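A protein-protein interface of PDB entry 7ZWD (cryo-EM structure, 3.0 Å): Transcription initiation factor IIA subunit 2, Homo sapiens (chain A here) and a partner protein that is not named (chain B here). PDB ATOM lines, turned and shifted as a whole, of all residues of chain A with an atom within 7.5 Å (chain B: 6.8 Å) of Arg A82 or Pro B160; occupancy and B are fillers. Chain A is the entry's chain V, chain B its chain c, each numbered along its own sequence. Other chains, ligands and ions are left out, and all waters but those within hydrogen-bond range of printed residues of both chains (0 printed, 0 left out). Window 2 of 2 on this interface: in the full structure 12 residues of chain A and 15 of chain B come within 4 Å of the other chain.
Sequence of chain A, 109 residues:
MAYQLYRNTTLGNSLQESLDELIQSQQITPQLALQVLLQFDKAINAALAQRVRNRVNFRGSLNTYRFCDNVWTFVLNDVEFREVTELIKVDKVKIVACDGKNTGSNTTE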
ATOM      1  N   ASN A  54      -2.653  -4.407  -1.731  1.00  0.00           N
ATOM      2  CA  ASN A  54      -2.132  -4.054  -3.040  1.00  0.00           C
ATOM      3  C   ASN A  54      -2.139  -5.312  -3.887  1.00  0.00           C
ATOM      4  O   ASN A  54      -1.667  -6.366  -3.466  1.00  0.00           O
ATOM      5  CB  ASN A  54      -0.730  -3.450  -2.957  1.00  0.00           C
ATOM      6  CG  ASN A  54       0.328  -4.472  -2.658  1.00  0.00           C
ATOM      7  OD1 ASN A  54       0.920  -5.052  -3.562  1.00  0.00           O
ATOM      8  ND2 ASN A  54       0.576  -4.700  -1.385  1.00  0.00           N
ATOM      9  N   ARG A  55      -2.694  -5.189  -5.082  1.00  0.00           N
ATOM     10  CA  ARG A  55      -2.883  -6.319  -5.969  1.00  0.00           C
ATOM     11  C   ARG A  55      -1.797  -6.328  -7.026  1.00  0.00           C
ATOM     12  O   ARG A  55      -1.522  -5.301  -7.650  1.00  0.00           O
ATOM     13  CB  ARG A  55      -4.250  -6.266  -6.638  1.00  0.00           C
ATOM     14  CG  ARG A  55      -4.594  -7.528  -7.385  1.00  0.00           C
ATOM     15  CD  ARG A  55      -5.931  -7.426  -8.084  1.00  0.00           C
ATOM     16  NE  ARG A  55      -5.819  -6.723  -9.356  1.00  0.00           N
ATOM     17  CZ  ARG A  55      -6.616  -6.936 -10.396  1.00  0.00           C
ATOM     18  NH1 ARG A  55      -7.585  -7.833 -10.315  1.00  0.00           N
ATOM     19  NH2 ARG A  55      -6.442  -6.253 -11.517  1.00  0.00           N
ATOM     20  N   VAL A  56      -1.175  -7.482  -7.223  1.00  0.00           N
ATOM     21  CA  VAL A  56      -0.249  -7.671  -8.325  1.00  0.00           C
ATOM     22  C   VAL A  56      -0.929  -8.562  -9.345  1.00  0.00           C
ATOM     23  O   VAL A  56      -1.951  -9.191  -9.061  1.00  0.00           O
ATOM     24  CB  VAL A  56       1.092  -8.283  -7.882  1.00  0.00           C
ATOM     25  CG1 VAL A  56       1.569  -7.627  -6.619  1.00  0.00           C
ATOM     26  CG2 VAL A  56       0.964  -9.756  -7.708  1.00  0.00           C
ATOM     27  N   ASN A  57      -0.373  -8.599 -10.547  1.00  0.00           N
ATOM     28  CA  ASN A  57      -0.863  -9.502 -11.574  1.00  0.00           C
ATOM     29  C   ASN A  57       0.344 -10.037 -12.311  1.00  0.00           C
ATOM     30  O   ASN A  57       1.145  -9.260 -12.821  1.00  0.00           O
ATOM     31  CB  ASN A  57      -1.791  -8.801 -12.563  1.00  0.00           C
ATOM     32  CG  ASN A  57      -2.796  -7.913 -11.890  1.00  0.00           C
ATOM     33  OD1 ASN A  57      -2.674  -6.696 -11.922  1.00  0.00           O
ATOM     34  ND2 ASN A  57      -3.805  -8.511 -11.287  1.00  0.00           N
ATOM     35  N   PHE A  58       0.493 -11.344 -12.361  1.00  0.00           N
ATOM     36  CA  PHE A  58       1.642 -11.893 -13.049  1.00  0.00           C
ATOM     37  C   PHE A  58       1.196 -12.737 -14.225  1.00  0.00           C
ATOM     38  O   PHE A  58       0.091 -13.272 -14.252  1.00  0.00           O
ATOM     39  CB  PHE A  58       2.536 -12.708 -12.120  1.00  0.00           C
ATOM     40  CG  PHE A  58       1.835 -13.811 -11.407  1.00  0.00           C
ATOM     41  CD1 PHE A  58       1.235 -13.590 -10.193  1.00  0.00           C
ATOM     42  CD2 PHE A  58       1.812 -15.081 -11.934  1.00  0.00           C
ATOM     43  CE1 PHE A  58       0.607 -14.602  -9.535  1.00  0.00           C
ATOM     44  CE2 PHE A  58       1.188 -16.092 -11.277  1.00  0.00           C
ATOM     45  CZ  PHE A  58       0.584 -15.854 -10.077  1.00  0.00           C
ATOM     46  N   ARG A  59       2.064 -12.803 -15.219  1.00  0.00           N
ATOM     47  CA  ARG A  59       1.892 -13.690 -16.354  1.00  0.00           C
ATOM     48  C   ARG A  59       3.196 -14.413 -16.606  1.00  0.00           C
ATOM     49  O   ARG A  59       4.261 -13.798 -16.611  1.00  0.00           O
ATOM     50  CB  ARG A  59       1.489 -12.940 -17.606  1.00  0.00           C
ATOM     51  CG  ARG A  59       0.035 -12.591 -17.684  1.00  0.00           C
ATOM     52  CD  ARG A  59      -0.421 -12.675 -19.116  1.00  0.00           C
ATOM     53  NE  ARG A  59      -1.239 -11.533 -19.492  1.00  0.00           N
ATOM     54  CZ  ARG A  59      -1.695 -11.324 -20.718  1.00  0.00           C
ATOM     55  NH1 ARG A  59      -1.411 -12.183 -21.687  1.00  0.00           N
ATOM     56  NH2 ARG A  59      -2.435 -10.258 -20.977  1.00  0.00           N
ATOM     57  N   GLU A  80       6.391 -12.086 -15.657  1.00  0.00           N
ATOM     58  CA  GLU A  80       6.350 -10.663 -15.375  1.00  0.00           C
ATOM     59  C   GLU A  80       5.285 -10.426 -14.321  1.00  0.00           C
ATOM     60  O   GLU A  80       4.115 -10.768 -14.524  1.00  0.00           O
ATOM     61  CB  GLU A  80       6.073  -9.843 -16.632  1.00  0.00           C
ATOM     62  CG  GLU A  80       4.771 -10.149 -17.312  1.00  0.00           C
ATOM     63  CD  GLU A  80       4.374  -9.071 -18.281  1.00  0.00           C
ATOM     64  OE1 GLU A  80       5.180  -8.760 -19.182  1.00  0.00           O
ATOM     65  OE2 GLU A  80       3.264  -8.520 -18.132  1.00  0.00           O
ATOM     66  N   PHE A  81       5.706  -9.908 -13.176  1.00  0.00           N
ATOM     67  CA  PHE A  81       4.808  -9.468 -12.129  1.00  0.00           C
ATOM     68  C   PHE A  81       4.522  -8.004 -12.354  1.00  0.00           C
ATOM     69  O   PHE A  81       5.380  -7.261 -12.833  1.00  0.00           O
ATOM     70  CB  PHE A  81       5.416  -9.675 -10.747  1.00  0.00           C
ATOM     71  CG  PHE A  81       5.630 -11.104 -10.406  1.00  0.00           C
ATOM     72  CD1 PHE A  81       4.735 -11.773  -9.609  1.00  0.00           C
ATOM     73  CD2 PHE A  81       6.715 -11.787 -10.901  1.00  0.00           C
ATOM     74  CE1 PHE A  81       4.923 -13.084  -9.308  1.00  0.00           C
ATOM     75  CE2 PHE A  81       6.904 -13.096 -10.600  1.00  0.00           C
ATOM     76  CZ  PHE A  81       6.009 -13.747  -9.804  1.00  0.00           C
ATOM     77  N   ARG A  82       3.319  -7.593 -12.012  1.00  0.00           N
ATOM     78  CA  ARG A  82       2.851  -6.258 -12.319  1.00  0.00           C
ATOM     79  C   ARG A  82       2.215  -5.710 -11.059  1.00  0.00           C
ATOM     80  O   ARG A  82       1.048  -5.998 -10.773  1.00  0.00           O
ATOM     81  CB  ARG A  82       1.867  -6.294 -13.475  1.00  0.00           C
ATOM     82  CG  ARG A  82       1.416  -4.953 -13.884  1.00  0.00           C
ATOM     83  CD  ARG A  82       2.572  -4.151 -14.403  1.00  0.00           C
ATOM     84  NE  ARG A  82       2.191  -2.755 -14.467  1.00  0.00           N
ATOM     85  CZ  ARG A  82       1.423  -2.257 -15.418  1.00  0.00           C
ATOM     86  NH1 ARG A  82       0.975  -3.047 -16.379  1.00  0.00           N
ATOM     87  NH2 ARG A  82       1.103  -0.975 -15.409  1.00  0.00           N
ATOM     88  N   GLU A  83       2.991  -4.946 -10.302  1.00  0.00           N
ATOM     89  CA  GLU A  83       2.497  -4.281  -9.110  1.00  0.00           C
ATOM     90  C   GLU A  83       1.750  -3.036  -9.563  1.00  0.00           C
ATOM     91  O   GLU A  83       1.350  -2.959 -10.725  1.00  0.00           O
ATOM     92  CB  GLU A  83       3.645  -3.967  -8.152  1.00  0.00           C
ATOM     93  CG  GLU A  83       3.205  -3.699  -6.723  1.00  0.00           C
ATOM     94  CD  GLU A  83       4.173  -4.243  -5.700  1.00  0.00           C
ATOM     95  OE1 GLU A  83       5.386  -3.980  -5.827  1.00  0.00           O
ATOM     96  OE2 GLU A  83       3.717  -4.929  -4.764  1.00  0.00           O
ATOM     97  N   VAL A  84       1.512  -2.088  -8.652  1.00  0.00           N
ATOM     98  CA  VAL A  84       0.652  -0.943  -8.942  1.00  0.00           C
ATOM     99  C   VAL A  84       0.944  -0.354 -10.320  1.00  0.00           C
ATOM    100  O   VAL A  84       0.048  -0.258 -11.164  1.00  0.00           O
ATOM    101  CB  VAL A  84       0.769   0.106  -7.817  1.00  0.00           C
ATOM    102  CG1 VAL A  84       2.211   0.530  -7.590  1.00  0.00           C
ATOM    103  CG2 VAL A  84      -0.089   1.314  -8.137  1.00  0.00           C
ATOM    104  N   THR A  85       2.191   0.026 -10.585  1.00  0.00           N
ATOM    105  CA  THR A  85       2.513   0.629 -11.872  1.00  0.00           C
ATOM    106  C   THR A  85       3.835   0.114 -12.418  1.00  0.00           C
ATOM    107  O   THR A  85       4.206   0.425 -13.552  1.00  0.00           O
ATOM    108  CB  THR A  85       2.566   2.147 -11.755  1.00  0.00           C
ATOM    109  OG1 THR A  85       2.642   2.716 -13.065  1.00  0.00           O
ATOM    110  CG2 THR A  85       3.791   2.563 -10.970  1.00  0.00           C
ATOM    111  N   GLU A  86       4.560  -0.653 -11.619  1.00  0.00           N
ATOM    112  CA  GLU A  86       5.904  -1.084 -11.963  1.00  0.00           C
ATOM    113  C   GLU A  86       5.887  -2.520 -12.456  1.00  0.00           C
ATOM    114  O   GLU A  86       5.050  -3.321 -12.038  1.00  0.00           O
ATOM    115  CB  GLU A  86       6.830  -0.958 -10.758  1.00  0.00           C
ATOM    116  CG  GLU A  86       6.234  -1.521  -9.491  1.00  0.00           C
ATOM    117  CD  GLU A  86       7.260  -1.711  -8.400  1.00  0.00           C
ATOM    118  OE1 GLU A  86       8.392  -2.134  -8.717  1.00  0.00           O
ATOM    119  OE2 GLU A  86       6.937  -1.440  -7.226  1.00  0.00           O
ATOM    120  N   LEU A  87       6.810  -2.835 -13.349  1.00  0.00           N
ATOM    121  CA  LEU A  87       6.986  -4.183 -13.855  1.00  0.00           C
ATOM    122  C   LEU A  87       8.171  -4.823 -13.155  1.00  0.00           C
ATOM    123  O   LEU A  87       9.192  -4.170 -12.928  1.00  0.00           O
ATOM    124  CB  LEU A  87       7.220  -4.171 -15.362  1.00  0.00           C
ATOM    125  CG  LEU A  87       6.810  -5.417 -16.135  1.00  0.00           C
ATOM    126  CD1 LEU A  87       5.331  -5.386 -16.431  1.00  0.00           C
ATOM    127  CD2 LEU A  87       7.597  -5.533 -17.419  1.00  0.00           C
ATOM    128  N   ILE A  88       8.036  -6.096 -12.805  1.00  0.00           N
ATOM    129  CA  ILE A  88       9.122  -6.875 -12.230  1.00  0.00           C
ATOM    130  C   ILE A  88       9.243  -8.152 -13.038  1.00  0.00           C
ATOM    131  O   ILE A  88       8.415  -9.053 -12.898  1.00  0.00           O
ATOM    132  CB  ILE A  88       8.879  -7.212 -10.749  1.00  0.00           C
ATOM    133  CG1 ILE A  88       8.657  -5.947  -9.927  1.00  0.00           C
ATOM    134  CG2 ILE A  88      10.043  -7.990 -10.195  1.00  0.00           C
ATOM    135  CD1 ILE A  88       7.230  -5.745  -9.504  1.00  0.00           C
ATOM    136  N   LYS A  89      10.258  -8.237 -13.880  1.00  0.00           N
ATOM    137  CA  LYS A  89      10.434  -9.394 -14.738  1.00  0.00           C
ATOM    138  C   LYS A  89      11.449 -10.337 -14.115  1.00  0.00           C
ATOM    139  O   LYS A  89      12.563  -9.929 -13.779  1.00  0.00           O
ATOM    140  CB  LYS A  89      10.891  -8.975 -16.132  1.00  0.00           C
ATOM    141  CG  LYS A  89      10.430  -9.904 -17.230  1.00  0.00           C
ATOM    142  CD  LYS A  89      10.704  -9.309 -18.598  1.00  0.00           C
ATOM    143  CE  LYS A  89      10.035 -10.121 -19.695  1.00  0.00           C
ATOM    144  NZ  LYS A  89      10.412 -11.559 -19.649  1.00  0.00           N
ATOM    145  N   ASP B 152      -4.936  -4.775 -20.631  1.00  0.00           N
ATOM    146  CA  ASP B 152      -5.060  -6.164 -21.036  1.00  0.00           C
ATOM    147  C   ASP B 152      -6.517  -6.540 -21.248  1.00  0.00           C
ATOM    148  O   ASP B 152      -7.409  -6.089 -20.530  1.00  0.00           O
ATOM    149  CB  ASP B 152      -4.477  -7.080 -19.966  1.00  0.00           C
ATOM    150  CG  ASP B 152      -2.988  -6.931 -19.813  1.00  0.00           C
ATOM    151  OD1 ASP B 152      -2.251  -7.766 -20.367  1.00  0.00           O
ATOM    152  OD2 ASP B 152      -2.549  -5.974 -19.146  1.00  0.00           O
ATOM    153  N   THR B 155      -6.098  -9.286 -17.911  1.00  0.00           N
ATOM    154  CA  THR B 155      -6.088  -8.773 -16.551  1.00  0.00           C
ATOM    155  C   THR B 155      -6.718  -7.398 -16.435  1.00  0.00           C
ATOM    156  O   THR B 155      -7.273  -7.069 -15.383  1.00  0.00           O
ATOM    157  CB  THR B 155      -4.657  -8.714 -16.029  1.00  0.00           C
ATOM    158  OG1 THR B 155      -3.999  -7.578 -16.596  1.00  0.00           O
ATOM    159  CG2 THR B 155      -3.901  -9.967 -16.424  1.00  0.00           C
ATOM    160  N   VAL B 157      -5.096  -4.342 -16.802  1.00  0.00           N
ATOM    161  CA  VAL B 157      -4.196  -3.353 -16.225  1.00  0.00           C
ATOM    162  C   VAL B 157      -3.402  -2.707 -17.346  1.00  0.00           C
ATOM    163  O   VAL B 157      -3.078  -3.355 -18.348  1.00  0.00           O
ATOM    164  CB  VAL B 157      -3.261  -3.977 -15.173  1.00  0.00           C
ATOM    165  CG1 VAL B 157      -4.074  -4.606 -14.073  1.00  0.00           C
ATOM    166  CG2 VAL B 157      -2.351  -4.998 -15.806  1.00  0.00           C
ATOM    167  N   GLY B 158      -3.094  -1.428 -17.182  1.00  0.00           N
ATOM    168  CA  GLY B 158      -2.391  -0.683 -18.193  1.00  0.00           C
ATOM    169  C   GLY B 158      -0.975  -1.172 -18.372  1.00  0.00           C
ATOM    170  O   GLY B 158      -0.530  -2.105 -17.705  1.00  0.00           O
ATOM    171  N   PRO B 159      -0.244  -0.566 -19.295  1.00  0.00           N
ATOM    172  CA  PRO B 159       1.171  -0.874 -19.429  1.00  0.00           C
ATOM    173  C   PRO B 159       1.949  -0.283 -18.270  1.00  0.00           C
ATOM    174  O   PRO B 159       1.417   0.552 -17.525  1.00  0.00           O
ATOM    175  CB  PRO B 159       1.548  -0.211 -20.759  1.00  0.00           C
ATOM    176  CG  PRO B 159       0.567   0.852 -20.937  1.00  0.00           C
ATOM    177  CD  PRO B 159      -0.703   0.388 -20.312  1.00  0.00           C
ATOM    178  N   PRO B 160       3.194  -0.700 -18.064  1.00  0.00           N
ATOM    179  CA  PRO B 160       3.986  -0.114 -16.984  1.00  0.00           C
ATOM    180  C   PRO B 160       4.190   1.375 -17.199  1.00  0.00           C
ATOM    181  O   PRO B 160       3.903   1.923 -18.262  1.00  0.00           O
ATOM    182  CB  PRO B 160       5.311  -0.875 -17.064  1.00  0.00           C
ATOM    183  CG  PRO B 160       5.345  -1.424 -18.430  1.00  0.00           C
ATOM    184  CD  PRO B 160       3.940  -1.744 -18.773  1.00  0.00           C
ATOM    185  N   ALA B 161       4.692   2.037 -16.165  1.00  0.00           N
ATOM    186  CA  ALA B 161       4.890   3.473 -16.243  1.00  0.00           C
ATOM    187  C   ALA B 161       6.018   3.810 -17.207  1.00  0.00           C
ATOM    188  O   ALA B 161       6.960   3.039 -17.389  1.00  0.00           O
ATOM    189  CB  ALA B 161       5.198   4.037 -14.859  1.00  0.00           C
ATOM    190  N   ASN B 162       5.916   4.982 -17.827  1.00  0.00           N
ATOM    191  CA  ASN B 162       6.981   5.504 -18.665  1.00  0.00           C
ATOM    192  C   ASN B 162       8.203   5.803 -17.811  1.00  0.00           C
ATOM    193  O   ASN B 162       8.186   5.678 -16.586  1.00  0.00           O
ATOM    194  CB  ASN B 162       6.536   6.778 -19.375  1.00  0.00           C
ATOM    195  CG  ASN B 162       5.247   6.606 -20.126  1.00  0.00           C
ATOM    196  OD1 ASN B 162       5.080   5.664 -20.894  1.00  0.00           O
ATOM    197  ND2 ASN B 162       4.317   7.520 -19.907  1.00  0.00           N
ATOM    198  N   THR B 165       7.101   9.158 -16.373  1.00  0.00           N
ATOM    199  CA  THR B 165       6.234   9.021 -15.209  1.00  0.00           C
ATOM    200  C   THR B 165       7.040   8.758 -13.951  1.00  0.00           C
ATOM    201  O   THR B 165       6.779   9.357 -12.903  1.00  0.00           O
ATOM    202  CB  THR B 165       5.232   7.898 -15.424  1.00  0.00           C
ATOM    203  OG1 THR B 165       4.546   8.102 -16.660  1.00  0.00           O
ATOM    204  CG2 THR B 165       4.238   7.885 -14.304  1.00  0.00           C
ATOM    205  N   ARG B 166       8.018   7.857 -14.027  1.00  0.00           N
ATOM    206  CA  ARG B 166       8.834   7.570 -12.856  1.00  0.00           C
ATOM    207  C   ARG B 166       9.638   8.790 -12.442  1.00  0.00           C
ATOM    208  O   ARG B 166       9.765   9.085 -11.251  1.00  0.00           O
ATOM    209  CB  ARG B 166       9.763   6.397 -13.135  1.00  0.00           C
ATOM    210  CG  ARG B 166       9.061   5.125 -13.522  1.00  0.00           C
ATOM    211  CD  ARG B 166      10.061   4.002 -13.665  1.00  0.00           C
ATOM    212  NE  ARG B 166       9.417   2.746 -14.028  1.00  0.00           N
ATOM    213  CZ  ARG B 166       9.590   2.128 -15.189  1.00  0.00           C
ATOM    214  NH1 ARG B 166      10.399   2.644 -16.104  1.00  0.00           N
ATOM    215  NH2 ARG B 166       8.961   0.988 -15.434  1.00  0.00           N
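Of the 10 printed residues of chain B, 6 touch a printed residue of chain A. Printed residues of chain B that touch a printed residue of chain A: Asp B152, Val B157, Gly B158, Pro B159, Pro B160 and Ala B161. Hydrophobic or aromatic side chains of chain B that line the printed part of chain A: Val B157, Pro B160 and Ala B161. Among the printed residues, 9 pairs touch across the chains. Among the printed residues, Asp or Glu carboxylates within 4 Å of a Lys or Arg side-chain nitrogen of the other chain: Arg A59 with Asp B152 (2.6 Å).
NH2 of Arg A82 lies close to N of Pro B160 (3.4 Å). The guanidinium group (NH2) of Arg A59 is in salt-bridge range of the side-chain carboxylate (OD1) of Asp B152 (2.6 Å). The backbone NH (N) of Ala B161 is in hydrogen-bond range of the backbone carbonyl oxygen (O) of Thr A85 (3.1 Å). The guanidinium group (NH2) of Arg A82 sits at hydrogen-bond distance from the backbone carbonyl oxygen (O) of Pro B159 (2.6 Å). The guanidinium group (NH2) of Arg A82 lies close to the backbone carbonyl oxygen (O) of Gly B158 (3.0 Å).
Among the printed residues, pairs that only touch across the chains: Arg A55 with Val B157 (3.9 Å), Asn A57 with Val B157 (3.3 Å), Arg A82 with Val B157 (3.9 Å) and Thr A85 with Pro B160 (3.5 Å).
Printed residues of chain B within 4 Å of Asn A57: Val B157. Ile A88 touches none of the printed residues of chain B. Of the printed residues of chain A, Gly B158 touches Arg A82. Printed residues of chain A within 4 Å of Ala B161: Thr A85. Thr B165 touches none of the printed residues of chain A. The nearest residue of chain A that does not touch Pro B160 is Leu A87 (4.2 Å).
The side-chain amide nitrogen (ND2) of Asn A57 lies close to the guanidinium group (NE) of Arg A55 (3.3 Å). The side-chain hydroxyl of Thr B155 sits close to the backbone NH of Val B157, 3.4 Å away. O of Ala B161 lies within hydrogen-bond range of NH2 of Arg B166 (3.5 Å). O of Arg A59 is in hydrogen-bond range of N of Glu A80, at 2.9 Å. N of Arg A82 lies within hydrogen-bond range of O of Asn A57 (2.9 Å). The side-chain carboxylate (OD2) of Asp B152 is in hydrogen-bond range of the side-chain hydroxyl (OG1) of Thr B155 (3.3 Å).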
